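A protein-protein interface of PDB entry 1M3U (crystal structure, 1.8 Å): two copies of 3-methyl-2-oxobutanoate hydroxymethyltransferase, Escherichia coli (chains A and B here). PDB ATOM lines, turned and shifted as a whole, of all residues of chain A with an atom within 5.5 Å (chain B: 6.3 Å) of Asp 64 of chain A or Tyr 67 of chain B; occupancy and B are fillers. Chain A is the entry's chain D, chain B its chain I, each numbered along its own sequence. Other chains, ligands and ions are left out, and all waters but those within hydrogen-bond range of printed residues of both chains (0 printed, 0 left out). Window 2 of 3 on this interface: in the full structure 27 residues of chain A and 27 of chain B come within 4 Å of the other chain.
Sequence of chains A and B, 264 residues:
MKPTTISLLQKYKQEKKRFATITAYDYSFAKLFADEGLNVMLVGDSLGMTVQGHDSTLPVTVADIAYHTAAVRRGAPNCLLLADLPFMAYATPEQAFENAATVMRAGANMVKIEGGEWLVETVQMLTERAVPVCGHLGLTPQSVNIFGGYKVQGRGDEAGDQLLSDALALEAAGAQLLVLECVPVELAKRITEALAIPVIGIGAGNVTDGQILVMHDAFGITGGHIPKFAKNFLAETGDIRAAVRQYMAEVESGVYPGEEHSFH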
ATOM      1  N   LEU A  47     -17.891   0.133  11.099  1.00  0.00           N
ATOM      2  CA  LEU A  47     -18.675   0.291   9.870  1.00  0.00           C
ATOM      3  C   LEU A  47     -19.196   1.705   9.615  1.00  0.00           C
ATOM      4  O   LEU A  47     -19.349   2.109   8.463  1.00  0.00           O
ATOM      5  CB  LEU A  47     -19.813  -0.735   9.840  1.00  0.00           C
ATOM      6  CG  LEU A  47     -21.072  -0.536  10.655  1.00  0.00           C
ATOM      7  CD1 LEU A  47     -22.100   0.427   9.982  1.00  0.00           C
ATOM      8  CD2 LEU A  47     -21.681  -1.877  10.959  1.00  0.00           C
ATOM      9  N   VAL A  51     -17.852   1.592   6.046  1.00  0.00           N
ATOM     10  CA  VAL A  51     -19.027   1.270   5.233  1.00  0.00           C
ATOM     11  C   VAL A  51     -19.846   2.522   4.918  1.00  0.00           C
ATOM     12  O   VAL A  51     -20.108   2.833   3.727  1.00  0.00           O
ATOM     13  CB  VAL A  51     -19.922   0.166   5.864  1.00  0.00           C
ATOM     14  CG1 VAL A  51     -21.212  -0.022   5.002  1.00  0.00           C
ATOM     15  CG2 VAL A  51     -19.164  -1.183   5.989  1.00  0.00           C
ATOM     16  N   GLN A  52     -20.225   3.261   5.961  1.00  0.00           N
ATOM     17  CA  GLN A  52     -21.110   4.419   5.794  1.00  0.00           C
ATOM     18  C   GLN A  52     -20.424   5.696   5.372  1.00  0.00           C
ATOM     19  O   GLN A  52     -21.031   6.558   4.710  1.00  0.00           O
ATOM     20  CB  GLN A  52     -21.951   4.660   7.069  1.00  0.00           C
ATOM     21  CG  GLN A  52     -22.745   3.442   7.531  1.00  0.00           C
ATOM     22  CD  GLN A  52     -23.450   3.685   8.810  1.00  0.00           C
ATOM     23  OE1 GLN A  52     -23.185   4.702   9.483  1.00  0.00           O
ATOM     24  NE2 GLN A  52     -24.401   2.793   9.161  1.00  0.00           N
ATOM     25  N   PRO A  59     -22.635   7.935  14.624  1.00  0.00           N
ATOM     26  CA  PRO A  59     -23.916   7.795  13.890  1.00  0.00           C
ATOM     27  C   PRO A  59     -24.424   6.395  13.689  1.00  0.00           C
ATOM     28  O   PRO A  59     -25.599   6.222  13.342  1.00  0.00           O
ATOM     29  CB  PRO A  59     -23.618   8.414  12.526  1.00  0.00           C
ATOM     30  CG  PRO A  59     -22.453   9.290  12.768  1.00  0.00           C
ATOM     31  CD  PRO A  59     -21.612   8.501  13.755  1.00  0.00           C
ATOM     32  N   VAL A  60     -23.603   5.389  13.930  1.00  0.00           N
ATOM     33  CA  VAL A  60     -24.052   4.012  13.769  1.00  0.00           C
ATOM     34  C   VAL A  60     -25.155   3.673  14.787  1.00  0.00           C
ATOM     35  O   VAL A  60     -25.027   3.937  16.001  1.00  0.00           O
ATOM     36  CB  VAL A  60     -22.862   2.998  13.901  1.00  0.00           C
ATOM     37  CG1 VAL A  60     -23.375   1.570  13.932  1.00  0.00           C
ATOM     38  CG2 VAL A  60     -21.884   3.195  12.791  1.00  0.00           C
ATOM     39  N   THR A  61     -26.242   3.091  14.291  1.00  0.00           N
ATOM     40  CA  THR A  61     -27.370   2.705  15.122  1.00  0.00           C
ATOM     41  C   THR A  61     -27.393   1.211  15.363  1.00  0.00           C
ATOM     42  O   THR A  61     -26.747   0.440  14.668  1.00  0.00           O
ATOM     43  CB  THR A  61     -28.750   3.091  14.503  1.00  0.00           C
ATOM     44  OG1 THR A  61     -28.954   2.337  13.306  1.00  0.00           O
ATOM     45  CG2 THR A  61     -28.845   4.555  14.096  1.00  0.00           C
ATOM     46  N   VAL A  62     -28.201   0.805  16.333  1.00  0.00           N
ATOM     47  CA  VAL A  62     -28.413  -0.618  16.627  1.00  0.00           C
ATOM     48  C   VAL A  62     -29.035  -1.277  15.394  1.00  0.00           C
ATOM     49  O   VAL A  62     -28.676  -2.377  15.035  1.00  0.00           O
ATOM     50  CB  VAL A  62     -29.353  -0.797  17.825  1.00  0.00           C
ATOM     51  CG1 VAL A  62     -29.761  -2.279  17.985  1.00  0.00           C
ATOM     52  CG2 VAL A  62     -28.683  -0.254  19.081  1.00  0.00           C
ATOM     53  N   ALA A  63     -29.944  -0.577  14.723  1.00  0.00           N
ATOM     54  CA  ALA A  63     -30.553  -1.113  13.499  1.00  0.00           C
ATOM     55  C   ALA A  63     -29.461  -1.383  12.450  1.00  0.00           C
ATOM     56  O   ALA A  63     -29.517  -2.385  11.748  1.00  0.00           O
ATOM     57  CB  ALA A  63     -31.600  -0.153  12.921  1.00  0.00           C
ATOM     58  N   ASP A  64     -28.461  -0.500  12.345  1.00  0.00           N
ATOM     59  CA  ASP A  64     -27.358  -0.676  11.377  1.00  0.00           C
ATOM     60  C   ASP A  64     -26.589  -1.951  11.711  1.00  0.00           C
ATOM     61  O   ASP A  64     -26.286  -2.766  10.833  1.00  0.00           O
ATOM     62  CB  ASP A  64     -26.355   0.497  11.374  1.00  0.00           C
ATOM     63  CG  ASP A  64     -26.938   1.806  10.943  1.00  0.00           C
ATOM     64  OD1 ASP A  64     -27.948   1.825  10.180  1.00  0.00           O
ATOM     65  OD2 ASP A  64     -26.427   2.905  11.331  1.00  0.00           O
ATOM     66  N   ILE A  65     -26.277  -2.120  13.001  1.00  0.00           N
ATOM     67  CA  ILE A  65     -25.494  -3.266  13.444  1.00  0.00           C
ATOM     68  C   ILE A  65     -26.288  -4.520  13.095  1.00  0.00           C
ATOM     69  O   ILE A  65     -25.729  -5.498  12.594  1.00  0.00           O
ATOM     70  CB  ILE A  65     -25.163  -3.203  14.957  1.00  0.00           C
ATOM     71  CG1 ILE A  65     -24.251  -2.008  15.245  1.00  0.00           C
ATOM     72  CG2 ILE A  65     -24.514  -4.514  15.399  1.00  0.00           C
ATOM     73  CD1 ILE A  65     -22.780  -2.120  14.655  1.00  0.00           C
ATOM     74  N   ALA A  66     -27.593  -4.492  13.337  1.00  0.00           N
ATOM     75  CA  ALA A  66     -28.422  -5.670  13.146  1.00  0.00           C
ATOM     76  C   ALA A  66     -28.491  -6.072  11.640  1.00  0.00           C
ATOM     77  O   ALA A  66     -28.600  -7.275  11.268  1.00  0.00           O
ATOM     78  CB  ALA A  66     -29.798  -5.429  13.703  1.00  0.00           C
ATOM     79  N   TYR A  67     -28.589  -5.051  10.790  1.00  0.00           N
ATOM     80  CA  TYR A  67     -28.581  -5.247   9.325  1.00  0.00           C
ATOM     81  C   TYR A  67     -27.315  -5.988   8.861  1.00  0.00           C
ATOM     82  O   TYR A  67     -27.379  -7.012   8.154  1.00  0.00           O
ATOM     83  CB  TYR A  67     -28.659  -3.886   8.660  1.00  0.00           C
ATOM     84  CG  TYR A  67     -28.576  -3.899   7.160  1.00  0.00           C
ATOM     85  CD1 TYR A  67     -29.635  -4.349   6.403  1.00  0.00           C
ATOM     86  CD2 TYR A  67     -27.442  -3.449   6.494  1.00  0.00           C
ATOM     87  CE1 TYR A  67     -29.540  -4.373   5.006  1.00  0.00           C
ATOM     88  CE2 TYR A  67     -27.355  -3.447   5.113  1.00  0.00           C
ATOM     89  CZ  TYR A  67     -28.427  -3.891   4.379  1.00  0.00           C
ATOM     90  OH  TYR A  67     -28.352  -3.880   3.027  1.00  0.00           O
ATOM     91  N   HIS A  68     -26.161  -5.488   9.303  1.00  0.00           N
ATOM     92  CA  HIS A  68     -24.870  -6.021   8.871  1.00  0.00           C
ATOM     93  C   HIS A  68     -24.609  -7.350   9.561  1.00  0.00           C
ATOM     94  O   HIS A  68     -23.996  -8.227   8.990  1.00  0.00           O
ATOM     95  CB  HIS A  68     -23.742  -5.024   9.112  1.00  0.00           C
ATOM     96  CG  HIS A  68     -23.778  -3.835   8.201  1.00  0.00           C
ATOM     97  ND1 HIS A  68     -23.342  -3.892   6.901  1.00  0.00           N
ATOM     98  CD2 HIS A  68     -24.253  -2.583   8.380  1.00  0.00           C
ATOM     99  CE1 HIS A  68     -23.513  -2.709   6.325  1.00  0.00           C
ATOM    100  NE2 HIS A  68     -24.085  -1.902   7.193  1.00  0.00           N
ATOM    101  N   THR A  69     -25.133  -7.525  10.772  1.00  0.00           N
ATOM    102  CA  THR A  69     -25.074  -8.812  11.493  1.00  0.00           C
ATOM    103  C   THR A  69     -25.802  -9.946  10.753  1.00  0.00           C
ATOM    104  O   THR A  69     -25.202 -10.999  10.568  1.00  0.00           O
ATOM    105  CB  THR A  69     -25.627  -8.631  12.922  1.00  0.00           C
ATOM    106  OG1 THR A  69     -24.702  -7.851  13.669  1.00  0.00           O
ATOM    107  CG2 THR A  69     -25.706  -9.943  13.681  1.00  0.00           C
ATOM    108  N   TYR B  25     -21.325  -0.363  -3.111  1.00  0.00           N
ATOM    109  CA  TYR B  25     -22.314  -0.404  -2.037  1.00  0.00           C
ATOM    110  C   TYR B  25     -21.846   0.175  -0.709  1.00  0.00           C
ATOM    111  O   TYR B  25     -22.589   0.138   0.272  1.00  0.00           O
ATOM    112  CB  TYR B  25     -22.830  -1.841  -1.819  1.00  0.00           C
ATOM    113  CG  TYR B  25     -23.012  -2.666  -3.089  1.00  0.00           C
ATOM    114  CD1 TYR B  25     -22.065  -3.620  -3.460  1.00  0.00           C
ATOM    115  CD2 TYR B  25     -24.133  -2.495  -3.912  1.00  0.00           C
ATOM    116  CE1 TYR B  25     -22.211  -4.382  -4.598  1.00  0.00           C
ATOM    117  CE2 TYR B  25     -24.283  -3.264  -5.082  1.00  0.00           C
ATOM    118  CZ  TYR B  25     -23.309  -4.206  -5.390  1.00  0.00           C
ATOM    119  OH  TYR B  25     -23.442  -4.971  -6.485  1.00  0.00           O
ATOM    120  N   VAL B  62     -36.420  -0.423  -1.069  1.00  0.00           N
ATOM    121  CA  VAL B  62     -36.049   0.949  -1.365  1.00  0.00           C
ATOM    122  C   VAL B  62     -35.210   1.561  -0.255  1.00  0.00           C
ATOM    123  O   VAL B  62     -34.242   2.217  -0.535  1.00  0.00           O
ATOM    124  CB  VAL B  62     -37.266   1.815  -1.673  1.00  0.00           C
ATOM    125  CG1 VAL B  62     -36.882   3.263  -1.852  1.00  0.00           C
ATOM    126  CG2 VAL B  62     -37.938   1.270  -2.920  1.00  0.00           C
ATOM    127  N   ALA B  63     -35.517   1.293   1.018  1.00  0.00           N
ATOM    128  CA  ALA B  63     -34.665   1.790   2.085  1.00  0.00           C
ATOM    129  C   ALA B  63     -33.247   1.214   2.066  1.00  0.00           C
ATOM    130  O   ALA B  63     -32.271   1.890   2.427  1.00  0.00           O
ATOM    131  CB  ALA B  63     -35.345   1.499   3.472  1.00  0.00           C
ATOM    132  N   ASP B  64     -33.123  -0.058   1.717  1.00  0.00           N
ATOM    133  CA  ASP B  64     -31.813  -0.674   1.504  1.00  0.00           C
ATOM    134  C   ASP B  64     -31.028   0.114   0.444  1.00  0.00           C
ATOM    135  O   ASP B  64     -29.850   0.495   0.645  1.00  0.00           O
ATOM    136  CB  ASP B  64     -31.949  -2.123   1.013  1.00  0.00           C
ATOM    137  CG  ASP B  64     -32.553  -3.056   2.032  1.00  0.00           C
ATOM    138  OD1 ASP B  64     -32.572  -2.758   3.280  1.00  0.00           O
ATOM    139  OD2 ASP B  64     -33.007  -4.150   1.651  1.00  0.00           O
ATOM    140  N   ILE B  65     -31.673   0.361  -0.697  1.00  0.00           N
ATOM    141  CA  ILE B  65     -31.000   1.097  -1.764  1.00  0.00           C
ATOM    142  C   ILE B  65     -30.539   2.466  -1.272  1.00  0.00           C
ATOM    143  O   ILE B  65     -29.411   2.871  -1.525  1.00  0.00           O
ATOM    144  CB  ILE B  65     -31.870   1.199  -3.045  1.00  0.00           C
ATOM    145  CG1 ILE B  65     -32.111  -0.206  -3.645  1.00  0.00           C
ATOM    146  CG2 ILE B  65     -31.225   2.195  -4.079  1.00  0.00           C
ATOM    147  CD1 ILE B  65     -30.943  -0.841  -4.288  1.00  0.00           C
ATOM    148  N   ALA B  66     -31.412   3.169  -0.584  1.00  0.00           N
ATOM    149  CA  ALA B  66     -31.127   4.521  -0.088  1.00  0.00           C
ATOM    150  C   ALA B  66     -29.984   4.510   0.899  1.00  0.00           C
ATOM    151  O   ALA B  66     -29.173   5.412   0.915  1.00  0.00           O
ATOM    152  CB  ALA B  66     -32.379   5.086   0.548  1.00  0.00           C
ATOM    153  N   TYR B  67     -29.929   3.491   1.753  1.00  0.00           N
ATOM    154  CA  TYR B  67     -28.825   3.346   2.710  1.00  0.00           C
ATOM    155  C   TYR B  67     -27.467   3.244   2.007  1.00  0.00           C
ATOM    156  O   TYR B  67     -26.527   3.978   2.284  1.00  0.00           O
ATOM    157  CB  TYR B  67     -29.060   2.097   3.549  1.00  0.00           C
ATOM    158  CG  TYR B  67     -27.945   1.727   4.506  1.00  0.00           C
ATOM    159  CD1 TYR B  67     -27.706   2.497   5.639  1.00  0.00           C
ATOM    160  CD2 TYR B  67     -27.196   0.584   4.328  1.00  0.00           C
ATOM    161  CE1 TYR B  67     -26.721   2.166   6.537  1.00  0.00           C
ATOM    162  CE2 TYR B  67     -26.178   0.237   5.217  1.00  0.00           C
ATOM    163  CZ  TYR B  67     -25.939   1.030   6.330  1.00  0.00           C
ATOM    164  OH  TYR B  67     -24.971   0.677   7.227  1.00  0.00           O
ATOM    165  N   HIS B  68     -27.374   2.324   1.064  1.00  0.00           N
ATOM    166  CA  HIS B  68     -26.164   2.137   0.299  1.00  0.00           C
ATOM    167  C   HIS B  68     -25.833   3.310  -0.601  1.00  0.00           C
ATOM    168  O   HIS B  68     -24.681   3.625  -0.822  1.00  0.00           O
ATOM    169  CB  HIS B  68     -26.226   0.813  -0.460  1.00  0.00           C
ATOM    170  CG  HIS B  68     -26.176  -0.360   0.457  1.00  0.00           C
ATOM    171  ND1 HIS B  68     -25.000  -0.812   1.000  1.00  0.00           N
ATOM    172  CD2 HIS B  68     -27.156  -1.138   0.971  1.00  0.00           C
ATOM    173  CE1 HIS B  68     -25.255  -1.835   1.797  1.00  0.00           C
ATOM    174  NE2 HIS B  68     -26.556  -2.039   1.819  1.00  0.00           N
ATOM    175  N   THR B  69     -26.859   3.964  -1.087  1.00  0.00           N
ATOM    176  CA  THR B  69     -26.685   5.086  -1.966  1.00  0.00           C
ATOM    177  C   THR B  69     -25.953   6.240  -1.251  1.00  0.00           C
ATOM    178  O   THR B  69     -24.992   6.816  -1.797  1.00  0.00           O
ATOM    179  CB  THR B  69     -28.062   5.499  -2.549  1.00  0.00           C
ATOM    180  OG1 THR B  69     -28.473   4.558  -3.555  1.00  0.00           O
ATOM    181  CG2 THR B  69     -27.964   6.852  -3.293  1.00  0.00           C
ATOM    182  N   ALA B  70     -26.422   6.583  -0.059  1.00  0.00           N
ATOM    183  CA  ALA B  70     -25.811   7.595   0.773  1.00  0.00           C
ATOM    184  C   ALA B  70     -24.329   7.285   1.048  1.00  0.00           C
ATOM    185  O   ALA B  70     -23.483   8.184   0.987  1.00  0.00           O
ATOM    186  CB  ALA B  70     -26.575   7.750   2.071  1.00  0.00           C
ATOM    187  N   ALA B  71     -24.025   6.043   1.401  1.00  0.00           N
ATOM    188  CA  ALA B  71     -22.652   5.593   1.633  1.00  0.00           C
ATOM    189  C   ALA B  71     -21.741   5.762   0.403  1.00  0.00           C
ATOM    190  O   ALA B  71     -20.637   6.275   0.496  1.00  0.00           O
ATOM    191  CB  ALA B  71     -22.681   4.126   2.062  1.00  0.00           C
ATOM    192  N   VAL B  72     -22.228   5.341  -0.760  1.00  0.00           N
ATOM    193  CA  VAL B  72     -21.487   5.479  -2.007  1.00  0.00           C
ATOM    194  C   VAL B  72     -21.266   6.961  -2.322  1.00  0.00           C
ATOM    195  O   VAL B  72     -20.171   7.330  -2.626  1.00  0.00           O
ATOM    196  CB  VAL B  72     -22.185   4.714  -3.179  1.00  0.00           C
ATOM    197  CG1 VAL B  72     -21.588   5.098  -4.543  1.00  0.00           C
ATOM    198  CG2 VAL B  72     -22.095   3.190  -2.940  1.00  0.00           C
ATOM    199  N   ARG B  74     -21.107   9.492  -0.252  1.00  0.00           N
ATOM    200  CA  ARG B  74     -20.049  10.022   0.613  1.00  0.00           C
ATOM    201  C   ARG B  74     -18.642   9.668   0.135  1.00  0.00           C
ATOM    202  O   ARG B  74     -17.723  10.464   0.294  1.00  0.00           O
ATOM    203  CB  ARG B  74     -20.209   9.582   2.078  1.00  0.00           C
ATOM    204  CG  ARG B  74     -21.359  10.200   2.781  1.00  0.00           C
ATOM    205  CD  ARG B  74     -21.529   9.737   4.196  1.00  0.00           C
ATOM    206  NE  ARG B  74     -22.884   9.944   4.650  1.00  0.00           N
ATOM    207  CZ  ARG B  74     -23.817   9.013   4.840  1.00  0.00           C
ATOM    208  NH1 ARG B  74     -23.583   7.676   4.695  1.00  0.00           N
ATOM    209  NH2 ARG B  74     -25.005   9.439   5.228  1.00  0.00           N
ATOM    210  N   ALA B 106     -31.396  10.631  -1.472  1.00  0.00           N
ATOM    211  CA  ALA B 106     -30.292   9.935  -0.754  1.00  0.00           C
ATOM    212  C   ALA B 106     -28.927  10.054  -1.460  1.00  0.00           C
ATOM    213  O   ALA B 106     -27.903   9.644  -0.919  1.00  0.00           O
ATOM    214  CB  ALA B 106     -30.645   8.478  -0.592  1.00  0.00           C
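The guanidinium group (NH1) of Arg 74 of chain B lies within hydrogen-bond range of the backbone carbonyl oxygen (O) of Gln 52 of chain A (2.8 Å).
NE2 of His 68 of chain A sits at hydrogen-bond distance from OH of Tyr 67 of chain B (2.7 Å).
The side-chain hydroxyl (OH) of Tyr 67 of chain A lies within hydrogen-bond range of a ring nitrogen (NE2) of His 68 of chain B (2.8 Å).
The side-chain amide nitrogen (NE2) of Gln 52 of chain A is in hydrogen-bond range of the side-chain hydroxyl (OH) of Tyr 67 of chain B (2.9 Å).
The backbone carbonyl oxygen of Leu 47 of chain A is in hydrogen-bond range of the backbone NH of Gln 52 of chain A (2.9 Å).
The backbone carbonyl oxygen (O) of Tyr 25 of chain B lies within hydrogen-bond range of a ring nitrogen (ND1) of His 68 of chain B, at 2.7 Å.
The side-chain amide nitrogen of Gln 52 of chain A is in hydrogen-bond range of the side-chain carboxylate of Asp 64 of chain A, at 3.0 Å.
The backbone NH (N) of Thr 61 of chain A is in hydrogen-bond range of the side-chain carboxylate (OD2) of Asp 64 of chain A, 3.0 Å away.
Among the printed residues, pairs that only touch across the chains: Leu 47 of chain A with Tyr 67 of chain B (3.99 Å), Val 51 of chain A with Ala 71 of chain B (3.3 Å), Gln 52 of chain A with Ala 71 of chain B (3.6 Å), Asp 64 of chain A with Tyr 67 of chain B (3.9 Å), Tyr 67 of chain A with Asp 64 of chain B (3.8 Å) and Tyr 67 of chain A with Tyr 67 of chain B (3.9 Å).
Of the printed residues of chain B, Val 51 of chain A touches Ala 71.
Of chain B, only Tyr 67 comes within 4 Å of Asp 64 of chain A.
Ile 65 of chain A touches none of the printed residues of chain B.
Ala 63 of chain B touches none of the printed residues of chain A.
Printed residues of chain A within 4 Å of Tyr 67 of chain B: Leu 47 (3.99 Å), Gln 52 (2.9 Å), Asp 64 (3.9 Å), Tyr 67 (3.9 Å) and His 68 (2.7 Å).
Of the printed residues of chain A, His 68 of chain B touches Tyr 67 (2.8 Å).
The nearest printed residue of chain B that does not touch Asp 64 of chain A is Arg 74 of chain B (8.7 Å).
The nearest printed residue of chain A that does not touch Tyr 67 of chain B is Val 51 of chain A (4.4 Å).
The nearest printed residue of chain B that does not touch Leu 47 of chain A is Ala 71 of chain B (7.5 Å).
Printed residues of chain B that touch a printed residue of chain A: Asp 64, Tyr 67, His 68, Ala 71 and Arg 74.
Hydrophobic or aromatic side chains of chain B that line the printed part of chain A: Tyr 67, His 68 and Ala 71.
Of the 14 printed residues of chain A, 6 touch a printed residue of chain B.
Among the printed residues, 10 pairs touch across the chains.
Among the printed residues, no Asp or Glu carboxylate lies within 4 Å of a Lys or Arg side-chain nitrogen of the other chain.
Asp 64 of chain A touches Tyr 67 of chain B, and with the chains exchanged Tyr 67 of chain A touches Asp 64 of chain B.
Tyr 67 of chain A touches its own counterpart, Tyr 67 of chain B.
Tyr 67 of chain A touches His 68 of chain B, and with the chains exchanged His 68 of chain A touches Tyr 67 of chain B.
Of the 10 pairs that touch across the chains among the printed residues, 5 have their exchanged pair printed and touching as well.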
